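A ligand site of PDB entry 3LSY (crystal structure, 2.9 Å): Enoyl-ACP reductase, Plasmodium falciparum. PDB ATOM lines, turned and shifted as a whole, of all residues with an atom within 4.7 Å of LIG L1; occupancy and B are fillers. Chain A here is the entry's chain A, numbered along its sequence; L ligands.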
ATOM      1  N   GLY A   9       7.530   1.958  13.337  1.00  0.00           N
ATOM      2  CA  GLY A   9       7.732   0.604  13.855  1.00  0.00           C
ATOM      3  C   GLY A   9       8.906  -0.172  13.296  1.00  0.00           C
ATOM      4  O   GLY A   9       8.744  -1.281  12.833  1.00  0.00           O
ATOM      5  N   ILE A  10      10.077   0.430  13.310  1.00  0.00           N
ATOM      6  CA  ILE A  10      11.299  -0.301  13.033  1.00  0.00           C
ATOM      7  C   ILE A  10      12.038  -0.424  14.345  1.00  0.00           C
ATOM      8  O   ILE A  10      11.909   0.444  15.223  1.00  0.00           O
ATOM      9  CB  ILE A  10      12.174   0.327  11.924  1.00  0.00           C
ATOM     10  CG1 ILE A  10      11.474   0.161  10.562  1.00  0.00           C
ATOM     11  CG2 ILE A  10      13.514  -0.384  11.810  1.00  0.00           C
ATOM     12  CD1 ILE A  10      12.190   0.798   9.375  1.00  0.00           C
ATOM     13  N   GLY A  11      12.748  -1.537  14.481  1.00  0.00           N
ATOM     14  CA  GLY A  11      13.664  -1.785  15.615  1.00  0.00           C
ATOM     15  C   GLY A  11      15.015  -2.362  15.179  1.00  0.00           C
ATOM     16  O   GLY A  11      16.002  -2.352  15.928  1.00  0.00           O
ATOM     17  N   ASP A  12      15.070  -2.841  13.944  1.00  0.00           N
ATOM     18  CA  ASP A  12      16.224  -3.540  13.433  1.00  0.00           C
ATOM     19  C   ASP A  12      15.866  -3.809  12.003  1.00  0.00           C
ATOM     20  O   ASP A  12      14.825  -3.345  11.547  1.00  0.00           O
ATOM     21  CB  ASP A  12      16.302  -4.908  14.079  1.00  0.00           C
ATOM     22  CG  ASP A  12      15.020  -5.662  13.910  1.00  0.00           C
ATOM     23  OD1 ASP A  12      14.012  -5.287  14.564  1.00  0.00           O
ATOM     24  OD2 ASP A  12      15.009  -6.584  13.095  1.00  0.00           O
ATOM     25  N   GLY A  15      12.704  -7.003   9.809  1.00  0.00           N
ATOM     26  CA  GLY A  15      11.277  -6.831   9.746  1.00  0.00           C
ATOM     27  C   GLY A  15      10.833  -6.335   8.407  1.00  0.00           C
ATOM     28  O   GLY A  15      11.646  -6.139   7.491  1.00  0.00           O
ATOM     29  N   TYR A  16       9.539  -6.157   8.266  1.00  0.00           N
ATOM     30  CA  TYR A  16       8.979  -5.672   7.019  1.00  0.00           C
ATOM     31  C   TYR A  16       9.225  -4.165   6.845  1.00  0.00           C
ATOM     32  O   TYR A  16       9.326  -3.678   5.729  1.00  0.00           O
ATOM     33  CB  TYR A  16       7.484  -5.993   6.946  1.00  0.00           C
ATOM     34  CG  TYR A  16       7.217  -7.416   6.530  1.00  0.00           C
ATOM     35  CD1 TYR A  16       7.580  -7.866   5.267  1.00  0.00           C
ATOM     36  CD2 TYR A  16       6.579  -8.312   7.398  1.00  0.00           C
ATOM     37  CE1 TYR A  16       7.336  -9.172   4.860  1.00  0.00           C
ATOM     38  CE2 TYR A  16       6.314  -9.638   6.981  1.00  0.00           C
ATOM     39  CZ  TYR A  16       6.709 -10.049   5.707  1.00  0.00           C
ATOM     40  OH  TYR A  16       6.475 -11.327   5.282  1.00  0.00           O
ATOM     41  N   GLY A  17       9.315  -3.437   7.958  1.00  0.00           N
ATOM     42  CA  GLY A  17       9.641  -2.022   7.900  1.00  0.00           C
ATOM     43  C   GLY A  17      10.945  -1.756   7.188  1.00  0.00           C
ATOM     44  O   GLY A  17      11.076  -0.765   6.467  1.00  0.00           O
ATOM     45  N   TRP A  36      10.266   2.759  18.415  1.00  0.00           N
ATOM     46  CA  TRP A  36       9.723   2.603  19.746  1.00  0.00           C
ATOM     47  C   TRP A  36      10.782   2.873  20.810  1.00  0.00           C
ATOM     48  O   TRP A  36      11.839   2.228  20.816  1.00  0.00           O
ATOM     49  CB  TRP A  36       9.232   1.171  19.880  1.00  0.00           C
ATOM     50  CG  TRP A  36       8.425   0.874  21.089  1.00  0.00           C
ATOM     51  CD1 TRP A  36       7.407   1.637  21.623  1.00  0.00           C
ATOM     52  CD2 TRP A  36       8.530  -0.295  21.921  1.00  0.00           C
ATOM     53  NE1 TRP A  36       6.890   1.017  22.742  1.00  0.00           N
ATOM     54  CE2 TRP A  36       7.563  -0.158  22.952  1.00  0.00           C
ATOM     55  CE3 TRP A  36       9.359  -1.425  21.897  1.00  0.00           C
ATOM     56  CZ2 TRP A  36       7.405  -1.126  23.944  1.00  0.00           C
ATOM     57  CZ3 TRP A  36       9.196  -2.371  22.888  1.00  0.00           C
ATOM     58  CH2 TRP A  36       8.218  -2.216  23.897  1.00  0.00           C
ATOM     59  N   VAL A  39      13.610   0.531  22.398  1.00  0.00           N
ATOM     60  CA  VAL A  39      14.740   0.073  21.560  1.00  0.00           C
ATOM     61  C   VAL A  39      15.491   1.140  20.740  1.00  0.00           C
ATOM     62  O   VAL A  39      16.450   0.813  20.066  1.00  0.00           O
ATOM     63  CB  VAL A  39      14.382  -1.178  20.707  1.00  0.00           C
ATOM     64  CG1 VAL A  39      13.867  -2.305  21.611  1.00  0.00           C
ATOM     65  CG2 VAL A  39      13.370  -0.865  19.613  1.00  0.00           C
ATOM     66  N   PHE A  72       9.338   7.141  18.838  1.00  0.00           N
ATOM     67  CA  PHE A  72       7.887   7.123  18.511  1.00  0.00           C
ATOM     68  C   PHE A  72       7.180   5.961  19.221  1.00  0.00           C
ATOM     69  O   PHE A  72       7.504   4.800  19.002  1.00  0.00           O
ATOM     70  CB  PHE A  72       7.656   7.008  16.979  1.00  0.00           C
ATOM     71  CG  PHE A  72       6.223   6.763  16.575  1.00  0.00           C
ATOM     72  CD1 PHE A  72       5.384   7.838  16.239  1.00  0.00           C
ATOM     73  CD2 PHE A  72       5.715   5.465  16.524  1.00  0.00           C
ATOM     74  CE1 PHE A  72       4.073   7.632  15.866  1.00  0.00           C
ATOM     75  CE2 PHE A  72       4.389   5.243  16.162  1.00  0.00           C
ATOM     76  CZ  PHE A  72       3.573   6.318  15.829  1.00  0.00           C
ATOM     77  N   ASP A  73       6.206   6.279  20.058  1.00  0.00           N
ATOM     78  CA  ASP A  73       5.468   5.259  20.786  1.00  0.00           C
ATOM     79  C   ASP A  73       3.980   5.385  20.526  1.00  0.00           C
ATOM     80  O   ASP A  73       3.363   6.357  20.941  1.00  0.00           O
ATOM     81  CB  ASP A  73       5.688   5.364  22.285  1.00  0.00           C
ATOM     82  CG  ASP A  73       5.184   4.143  23.014  1.00  0.00           C
ATOM     83  OD1 ASP A  73       4.131   3.602  22.606  1.00  0.00           O
ATOM     84  OD2 ASP A  73       5.832   3.704  23.989  1.00  0.00           O
ATOM     85  N   ALA A  74       3.420   4.375  19.879  1.00  0.00           N
ATOM     86  CA  ALA A  74       2.079   4.430  19.325  1.00  0.00           C
ATOM     87  C   ALA A  74       1.041   4.227  20.392  1.00  0.00           C
ATOM     88  O   ALA A  74      -0.168   4.225  20.117  1.00  0.00           O
ATOM     89  CB  ALA A  74       1.940   3.390  18.237  1.00  0.00           C
ATOM     90  N   SER A  75       1.516   4.024  21.616  1.00  0.00           N
ATOM     91  CA  SER A  75       0.660   3.981  22.800  1.00  0.00           C
ATOM     92  C   SER A  75       0.036   5.338  23.102  1.00  0.00           C
ATOM     93  O   SER A  75      -1.051   5.375  23.647  1.00  0.00           O
ATOM     94  CB  SER A  75       1.424   3.480  24.035  1.00  0.00           C
ATOM     95  OG  SER A  75       1.966   2.183  23.868  1.00  0.00           O
ATOM     96  N   SER A 120       3.518  -0.167  10.650  1.00  0.00           N
ATOM     97  CA  SER A 120       4.248  -1.398  10.565  1.00  0.00           C
ATOM     98  C   SER A 120       4.640  -1.861  11.926  1.00  0.00           C
ATOM     99  O   SER A 120       5.763  -2.321  12.130  1.00  0.00           O
ATOM    100  CB  SER A 120       5.511  -1.143   9.764  1.00  0.00           C
ATOM    101  OG  SER A 120       6.204  -2.359   9.551  1.00  0.00           O
ATOM    102  N   LEU A 121       3.696  -1.731  12.865  1.00  0.00           N
ATOM    103  CA  LEU A 121       3.908  -2.119  14.250  1.00  0.00           C
ATOM    104  C   LEU A 121       2.725  -2.912  14.733  1.00  0.00           C
ATOM    105  O   LEU A 121       1.583  -2.614  14.388  1.00  0.00           O
ATOM    106  CB  LEU A 121       4.115  -0.894  15.147  1.00  0.00           C
ATOM    107  CG  LEU A 121       2.990   0.155  15.084  1.00  0.00           C
ATOM    108  CD1 LEU A 121       2.082   0.071  16.309  1.00  0.00           C
ATOM    109  CD2 LEU A 121       3.571   1.554  14.911  1.00  0.00           C
ATOM    110  N   ALA A 122       3.016  -3.912  15.546  1.00  0.00           N
ATOM    111  CA  ALA A 122       2.042  -4.721  16.244  1.00  0.00           C
ATOM    112  C   ALA A 122       2.640  -5.023  17.609  1.00  0.00           C
ATOM    113  O   ALA A 122       3.876  -5.085  17.770  1.00  0.00           O
ATOM    114  CB  ALA A 122       1.781  -5.997  15.501  1.00  0.00           C
ATOM    115  N   ASN A 123       1.774  -5.179  18.608  1.00  0.00           N
ATOM    116  CA  ASN A 123       2.182  -5.477  19.986  1.00  0.00           C
ATOM    117  C   ASN A 123       1.018  -6.016  20.816  1.00  0.00           C
ATOM    118  O   ASN A 123      -0.057  -5.412  20.859  1.00  0.00           O
ATOM    119  CB  ASN A 123       2.802  -4.246  20.652  1.00  0.00           C
ATOM    120  CG  ASN A 123       3.761  -4.600  21.788  1.00  0.00           C
ATOM    121  OD1 ASN A 123       4.257  -3.721  22.485  1.00  0.00           O
ATOM    122  ND2 ASN A 123       4.017  -5.898  21.972  1.00  0.00           N
ATOM    123  N   LYS A 145      -2.519  -0.807  20.675  1.00  0.00           N
ATOM    124  CA  LYS A 145      -1.234  -0.600  20.031  1.00  0.00           C
ATOM    125  C   LYS A 145      -1.198  -1.032  18.558  1.00  0.00           C
ATOM    126  O   LYS A 145      -0.502  -0.424  17.724  1.00  0.00           O
ATOM    127  CB  LYS A 145      -0.149  -1.260  20.867  1.00  0.00           C
ATOM    128  CG  LYS A 145      -0.141  -0.663  22.253  1.00  0.00           C
ATOM    129  CD  LYS A 145       0.666  -1.460  23.262  1.00  0.00           C
ATOM    130  CE  LYS A 145       0.944  -0.604  24.489  1.00  0.00           C
ATOM    131  NZ  LYS A 145       2.112  -1.200  25.198  1.00  0.00           N
ATOM    132  N   LEU A 170       0.272  -3.322   7.695  1.00  0.00           N
ATOM    133  CA  LEU A 170       0.465  -4.730   7.397  1.00  0.00           C
ATOM    134  C   LEU A 170      -0.477  -5.558   8.235  1.00  0.00           C
ATOM    135  O   LEU A 170      -0.688  -5.224   9.405  1.00  0.00           O
ATOM    136  CB  LEU A 170       1.898  -5.118   7.690  1.00  0.00           C
ATOM    137  CG  LEU A 170       2.960  -4.454   6.823  1.00  0.00           C
ATOM    138  CD1 LEU A 170       4.267  -4.308   7.577  1.00  0.00           C
ATOM    139  CD2 LEU A 170       3.180  -5.249   5.543  1.00  0.00           C
ATOM    140  N   THR A 171      -1.052  -6.620   7.667  1.00  0.00           N
ATOM    141  CA  THR A 171      -2.004  -7.457   8.414  1.00  0.00           C
ATOM    142  C   THR A 171      -1.666  -8.936   8.271  1.00  0.00           C
ATOM    143  O   THR A 171      -0.695  -9.265   7.603  1.00  0.00           O
ATOM    144  CB  THR A 171      -3.502  -7.105   8.068  1.00  0.00           C
ATOM    145  OG1 THR A 171      -4.425  -7.972   8.758  1.00  0.00           O
ATOM    146  CG2 THR A 171      -3.764  -7.170   6.567  1.00  0.00           C
ATOM    147  N   TYR A 172      -2.421  -9.825   8.904  1.00  0.00           N
ATOM    148  CA  TYR A 172      -2.204 -11.236   8.732  1.00  0.00           C
ATOM    149  C   TYR A 172      -3.528 -11.937   8.475  1.00  0.00           C
ATOM    150  O   TYR A 172      -4.579 -11.544   9.016  1.00  0.00           O
ATOM    151  CB  TYR A 172      -1.517 -11.810   9.952  1.00  0.00           C
ATOM    152  CG  TYR A 172      -1.158 -13.262   9.853  1.00  0.00           C
ATOM    153  CD1 TYR A 172      -0.294 -13.707   8.881  1.00  0.00           C
ATOM    154  CD2 TYR A 172      -1.660 -14.185  10.756  1.00  0.00           C
ATOM    155  CE1 TYR A 172       0.055 -15.061   8.777  1.00  0.00           C
ATOM    156  CE2 TYR A 172      -1.320 -15.533  10.692  1.00  0.00           C
ATOM    157  CZ  TYR A 172      -0.466 -15.968   9.694  1.00  0.00           C
ATOM    158  OH  TYR A 172      -0.122 -17.310   9.584  1.00  0.00           O
ATOM    159  N   TYR A 182      -1.741 -17.877  17.321  1.00  0.00           N
ATOM    160  CA  TYR A 182      -1.755 -16.409  17.152  1.00  0.00           C
ATOM    161  C   TYR A 182      -2.709 -15.816  18.169  1.00  0.00           C
ATOM    162  O   TYR A 182      -3.812 -15.397  17.850  1.00  0.00           O
ATOM    163  CB  TYR A 182      -2.209 -16.074  15.726  1.00  0.00           C
ATOM    164  CG  TYR A 182      -1.861 -14.682  15.170  1.00  0.00           C
ATOM    165  CD1 TYR A 182      -0.573 -14.367  14.746  1.00  0.00           C
ATOM    166  CD2 TYR A 182      -2.843 -13.724  15.003  1.00  0.00           C
ATOM    167  CE1 TYR A 182      -0.282 -13.128  14.217  1.00  0.00           C
ATOM    168  CE2 TYR A 182      -2.569 -12.472  14.463  1.00  0.00           C
ATOM    169  CZ  TYR A 182      -1.298 -12.171  14.075  1.00  0.00           C
ATOM    170  OH  TYR A 182      -1.042 -10.932  13.538  1.00  0.00           O
ATOM    171  N   MET A 186      -4.362 -10.678  18.826  1.00  0.00           N
ATOM    172  CA  MET A 186      -3.771 -10.194  17.569  1.00  0.00           C
ATOM    173  C   MET A 186      -4.669 -10.549  16.361  1.00  0.00           C
ATOM    174  O   MET A 186      -4.819  -9.764  15.435  1.00  0.00           O
ATOM    175  CB  MET A 186      -2.385 -10.793  17.338  1.00  0.00           C
ATOM    176  CG  MET A 186      -1.230 -10.095  17.999  1.00  0.00           C
ATOM    177  SD  MET A 186      -1.260  -8.293  17.852  1.00  0.00           S
ATOM    178  CE  MET A 186      -1.191  -7.981  16.093  1.00  0.00           C
ATOM    179  N   LYS A 190      -5.947  -7.670  14.179  1.00  0.00           N
ATOM    180  CA  LYS A 190      -5.873  -7.702  12.729  1.00  0.00           C
ATOM    181  C   LYS A 190      -7.270  -7.611  12.098  1.00  0.00           C
ATOM    182  O   LYS A 190      -7.439  -6.960  11.041  1.00  0.00           O
ATOM    183  CB  LYS A 190      -5.119  -8.933  12.256  1.00  0.00           C
ATOM    184  CG  LYS A 190      -3.635  -8.932  12.575  1.00  0.00           C
ATOM    185  CD  LYS A 190      -2.919  -7.711  12.076  1.00  0.00           C
ATOM    186  CE  LYS A 190      -1.457  -7.722  12.479  1.00  0.00           C
ATOM    187  NZ  LYS A 190      -0.688  -6.541  11.897  1.00  0.00           N
ATOM    188  N   ALA A 217       0.774  -9.954   4.731  1.00  0.00           N
ATOM    189  CA  ALA A 217       2.049 -10.647   4.503  1.00  0.00           C
ATOM    190  C   ALA A 217       2.105 -12.058   5.063  1.00  0.00           C
ATOM    191  O   ALA A 217       1.549 -12.332   6.140  1.00  0.00           O
ATOM    192  CB  ALA A 217       3.172  -9.851   5.098  1.00  0.00           C
ATOM    193  N   GLY A 218       2.799 -12.940   4.340  1.00  0.00           N
ATOM    194  CA  GLY A 218       3.083 -14.303   4.809  1.00  0.00           C
ATOM    195  C   GLY A 218       4.121 -14.251   5.906  1.00  0.00           C
ATOM    196  O   GLY A 218       4.500 -13.168   6.359  1.00  0.00           O
ATOM    197  N   PRO A 219       4.629 -15.402   6.333  1.00  0.00           N
ATOM    198  CA  PRO A 219       5.455 -15.358   7.529  1.00  0.00           C
ATOM    199  C   PRO A 219       6.886 -14.905   7.219  1.00  0.00           C
ATOM    200  O   PRO A 219       7.410 -15.135   6.136  1.00  0.00           O
ATOM    201  CB  PRO A 219       5.429 -16.802   8.021  1.00  0.00           C
ATOM    202  CG  PRO A 219       4.862 -17.641   6.843  1.00  0.00           C
ATOM    203  CD  PRO A 219       4.697 -16.712   5.677  1.00  0.00           C
ATOM    204  N   LEU A 220       7.478 -14.224   8.170  1.00  0.00           N
ATOM    205  CA  LEU A 220       8.826 -13.737   8.010  1.00  0.00           C
ATOM    206  C   LEU A 220       9.480 -13.806   9.388  1.00  0.00           C
ATOM    207  O   LEU A 220       8.914 -13.271  10.368  1.00  0.00           O
ATOM    208  CB  LEU A 220       8.801 -12.297   7.493  1.00  0.00           C
ATOM    209  CG  LEU A 220      10.140 -11.639   7.191  1.00  0.00           C
ATOM    210  CD1 LEU A 220      10.907 -12.399   6.103  1.00  0.00           C
ATOM    211  CD2 LEU A 220       9.945 -10.179   6.845  1.00  0.00           C
ATOM    212  N   SER A 222      11.047 -12.578  11.926  1.00  0.00           N
ATOM    213  CA  SER A 222      11.411 -11.278  12.428  1.00  0.00           C
ATOM    214  C   SER A 222      11.564 -11.362  13.935  1.00  0.00           C
ATOM    215  O   SER A 222      11.251 -12.397  14.545  1.00  0.00           O
ATOM    216  CB  SER A 222      10.336 -10.252  12.096  1.00  0.00           C
ATOM    217  OG  SER A 222       9.216 -10.396  12.967  1.00  0.00           O
ATOM    218  N   ARG A 223      12.042 -10.269  14.520  1.00  0.00           N
ATOM    219  CA  ARG A 223      12.123 -10.143  15.971  1.00  0.00           C
ATOM    220  C   ARG A 223      10.802 -10.537  16.622  1.00  0.00           C
ATOM    221  O   ARG A 223      10.752 -11.477  17.418  1.00  0.00           O
ATOM    222  N   ALA A 224       9.739  -9.824  16.242  1.00  0.00           N
ATOM    223  CA  ALA A 224       8.412  -9.998  16.847  1.00  0.00           C
ATOM    224  C   ALA A 224       7.822 -11.407  16.654  1.00  0.00           C
ATOM    225  O   ALA A 224       7.167 -11.932  17.557  1.00  0.00           O
ATOM    226  CB  ALA A 224       7.441  -8.950  16.307  1.00  0.00           C
ATOM    227  N   ALA A 225       8.084 -11.996  15.486  1.00  0.00           N
ATOM    228  CA  ALA A 225       7.612 -13.323  15.123  1.00  0.00           C
ATOM    229  C   ALA A 225       8.086 -14.389  16.109  1.00  0.00           C
ATOM    230  O   ALA A 225       7.336 -15.302  16.469  1.00  0.00           O
ATOM    231  CB  ALA A 225       8.057 -13.663  13.727  1.00  0.00           C
ATOM    232  N   ILE A 274       6.685 -19.434  14.440  1.00  0.00           N
ATOM    233  CA  ILE A 274       7.057 -18.772  13.214  1.00  0.00           C
ATOM    234  C   ILE A 274       7.931 -19.673  12.316  1.00  0.00           C
ATOM    235  O   ILE A 274       7.998 -19.463  11.104  1.00  0.00           O
ATOM    236  CB  ILE A 274       7.703 -17.409  13.539  1.00  0.00           C
ATOM    237  CG1 ILE A 274       7.253 -16.334  12.535  1.00  0.00           C
ATOM    238  CG2 ILE A 274       9.224 -17.532  13.740  1.00  0.00           C
ATOM    239  CD1 ILE A 274       7.933 -16.356  11.185  1.00  0.00           C
HETATM  240  P1  LIG L   1       9.088  -6.130  13.877  1.00  0.00           P
HETATM  241  O1  LIG L   1       9.416  -6.412  15.341  1.00  0.00           O
HETATM  242  O2  LIG L   1      10.200  -6.210  12.861  1.00  0.00           O
HETATM  243  O3  LIG L   1       8.409  -4.674  13.746  1.00  0.00           O
HETATM  244  C1  LIG L   1       7.435  -4.251  14.700  1.00  0.00           C
HETATM  245  C2  LIG L   1       8.012  -3.078  15.455  1.00  0.00           C
HETATM  246  O4  LIG L   1       6.965  -2.304  16.039  1.00  0.00           O
HETATM  247  C3  LIG L   1       8.900  -3.548  16.603  1.00  0.00           C
HETATM  248  O5  LIG L   1      10.276  -3.427  16.198  1.00  0.00           O
HETATM  249  C4  LIG L   1       8.600  -2.624  17.757  1.00  0.00           C
HETATM  250  O6  LIG L   1       9.764  -1.845  18.065  1.00  0.00           O
HETATM  251  C5  LIG L   1       7.514  -1.684  17.227  1.00  0.00           C
HETATM  252  N1  LIG L   1       6.509  -1.402  18.292  1.00  0.00           N
HETATM  253  C6  LIG L   1       5.952  -2.306  19.111  1.00  0.00           C
HETATM  254  N2  LIG L   1       5.086  -1.688  19.962  1.00  0.00           N
HETATM  255  C7  LIG L   1       5.133  -0.371  19.668  1.00  0.00           C
HETATM  256  C8  LIG L   1       4.447   0.822  20.224  1.00  0.00           C
HETATM  257  N3  LIG L   1       3.571   0.683  21.234  1.00  0.00           N
HETATM  258  N4  LIG L   1       4.700   2.028  19.689  1.00  0.00           N
HETATM  259  C9  LIG L   1       5.578   2.139  18.668  1.00  0.00           C
HETATM  260  N5  LIG L   1       6.227   1.064  18.135  1.00  0.00           N
HETATM  261  C10 LIG L   1       6.017  -0.183  18.616  1.00  0.00           C
HETATM  262  O7  LIG L   1       7.861  -7.118  13.430  1.00  0.00           O
HETATM  263  P2  LIG L   1       7.526  -7.501  11.881  1.00  0.00           P
HETATM  264  O8  LIG L   1       7.649  -9.020  11.779  1.00  0.00           O
HETATM  265  O9  LIG L   1       8.270  -6.578  10.932  1.00  0.00           O
HETATM  266  O10 LIG L   1       5.990  -7.090  11.766  1.00  0.00           O
HETATM  267  C11 LIG L   1       5.613  -5.815  11.259  1.00  0.00           C
HETATM  268  C12 LIG L   1       4.098  -5.857  11.042  1.00  0.00           C
HETATM  269  O11 LIG L   1       3.775  -6.818  10.026  1.00  0.00           O
HETATM  270  C13 LIG L   1       3.408  -6.336  12.298  1.00  0.00           C
HETATM  271  O12 LIG L   1       2.400  -5.378  12.633  1.00  0.00           O
HETATM  272  C14 LIG L   1       2.735  -7.661  12.009  1.00  0.00           C
HETATM  273  O13 LIG L   1       1.405  -7.596  12.553  1.00  0.00           O
HETATM  274  C15 LIG L   1       2.742  -7.727  10.473  1.00  0.00           C
HETATM  275  N6  LIG L   1       2.935  -9.102   9.948  1.00  0.00           N
HETATM  276  C16 LIG L   1       4.082  -9.752  10.234  1.00  0.00           C
HETATM  277  C17 LIG L   1       4.353 -11.038   9.799  1.00  0.00           C
HETATM  278  C18 LIG L   1       5.665 -11.693  10.151  1.00  0.00           C
HETATM  279  O14 LIG L   1       5.858 -12.878   9.944  1.00  0.00           O
HETATM  280  N7  LIG L   1       6.627 -10.968  10.709  1.00  0.00           N
HETATM  281  C19 LIG L   1       3.301 -11.758   8.961  1.00  0.00           C
HETATM  282  C20 LIG L   1       2.080 -10.961   8.700  1.00  0.00           C
HETATM  283  C21 LIG L   1       1.955  -9.674   9.212  1.00  0.00           C
HETATM  284  C1  LG2 L   2       3.421 -10.751  13.865  1.00  0.00           C
HETATM  285  C2  LG2 L   2       2.260 -11.049  13.167  1.00  0.00           C
HETATM  286  C3  LG2 L   2       2.161 -12.236  12.443  1.00  0.00           C
HETATM  287  C4  LG2 L   2       3.227 -13.130  12.426  1.00  0.00           C
HETATM  288  C5  LG2 L   2       4.405 -12.846  13.135  1.00  0.00           C
HETATM  289  C6  LG2 L   2       4.500 -11.646  13.854  1.00  0.00           C
HETATM  290  O1  LG2 L   2       3.458  -9.560  14.571  1.00  0.00           O
HETATM  291  C7  LG2 L   2       3.308  -9.566  15.936  1.00  0.00           C
HETATM  292  C8  LG2 L   2       3.689  -8.455  16.684  1.00  0.00           C
HETATM  293  C9  LG2 L   2       3.550  -8.470  18.076  1.00  0.00           C
HETATM  294  C10 LG2 L   2       3.032  -9.589  18.733  1.00  0.00           C
HETATM  295  C11 LG2 L   2       2.657 -10.704  17.969  1.00  0.00           C
HETATM  296  C12 LG2 L   2       2.787 -10.691  16.581  1.00  0.00           C
HETATM  297  C13 LG2 L   2       3.098 -14.391  11.666  1.00  0.00           C
HETATM  298  O2  LG2 L   2       3.844 -14.547  10.733  1.00  0.00           O
HETATM  299  O3  LG2 L   2       1.233 -10.168  13.196  1.00  0.00           O
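OG of Ser 222 sits at hydrogen-bond distance from O8 of LIG L1 (2.4 Å).
The side-chain amino group of Lys 190 sits at hydrogen-bond distance from an oxygen (O13) of LIG L1 (2.4 Å).
The backbone NH (N) of Ala 74 is in hydrogen-bond range of a nitrogen (N4) of LIG L1, at 2.7 Å.
An oxygen (O14) of LIG L1 sits at hydrogen-bond distance from the backbone NH (N) of Leu 220, 2.8 Å away.
N7 of LIG L1 sits at hydrogen-bond distance from O of Leu 220 (3.3 Å).
The backbone NH (N) of Tyr 16 is in hydrogen-bond range of an oxygen (O9) of LIG L1 (3.0 Å).
The backbone NH (N) of Ala 122 lies close to an oxygen (O12) of LIG L1, 3.3 Å away.
The backbone carbonyl oxygen (O) of Leu 121 lies close to an oxygen (O12) of LIG L1 (3.4 Å).
A nitrogen (N3) of LIG L1 is in hydrogen-bond range of the side-chain carboxylate (OD1) of Asp 73, 3.3 Å away.
The side-chain amide oxygen of Asn 123 sits close to a nitrogen (N2) of LIG L1.
The side-chain hydroxyl (OG) of Ser 75 sits at hydrogen-bond distance from a nitrogen (N3) of LIG L1, 3.4 Å away.
An oxygen (O3) of LG2 L2 is in hydrogen-bond range of the side-chain hydroxyl of Tyr 182, 2.4 Å away.
O3 of LG2 L2 is in hydrogen-bond range of O13 of LIG L1 (2.7 Å).
N of Ala 224 sits close to OG of Ser 222 (3.4 Å).
N of Ala 225 sits at hydrogen-bond distance from OG of Ser 222.
The side-chain amino group of Lys 190 is in hydrogen-bond range of the backbone carbonyl oxygen of Leu 170 (2.8 Å).
O of Thr 171 lies within hydrogen-bond range of N of Ala 217 (3.3 Å).
The side-chain hydroxyl (OH) of Tyr 16 is in hydrogen-bond range of the backbone carbonyl oxygen (O) of Gly 218, at 2.9 Å.
The side-chain carboxylate (OD2) of Asp 73 is in hydrogen-bond range of the indole nitrogen (NE1) of Trp 36 (3.1 Å).
The backbone NH (N) of Ser 75 sits at hydrogen-bond distance from the side-chain carboxylate (OD1) of Asp 73, at 2.8 Å.
N of Trp 36 lies close to O of Phe 72 (3.5 Å).
Residues that only touch LIG L1: Gly 9 (3.3 Å), Ile 10 (3.9 Å), Gly 11 (3.6 Å), Gly 15 (3.2 Å), Trp 36 (3.3 Å), Phe 72 (3.3 Å), Ser 120 (3.6 Å), Leu 170 (3.4 Å), Thr 171 (3.1 Å), Tyr 172 (3.6 Å), Ala 217 (3.0 Å), Gly 218 (3.2 Å), Pro 219 (3.5 Å) and Ala 224 (3.4 Å).
Hydrophobic or aromatic side chains within 4 Å of LIG L1: Tyr 16, Trp 36, Phe 72, Ala 74, Leu 121, Ala 122, Leu 170, Tyr 172, Ala 217, Leu 220 and Ala 224.
Within 4 Å of LIG L1: Gly 9, Ile 10, Gly 11, Gly 15, Tyr 16, Trp 36, Phe 72, Asp 73, Ala 74, Ser 75, Ser 120, Leu 121, Ala 122, Asn 123, Leu 170, Thr 171, Tyr 172, Lys 190, Ala 217, Gly 218, Pro 219, Leu 220, Ser 222 and Ala 224.
The nearest printed residue that does not touch LIG L1 is Val 39 (4.04 Å).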
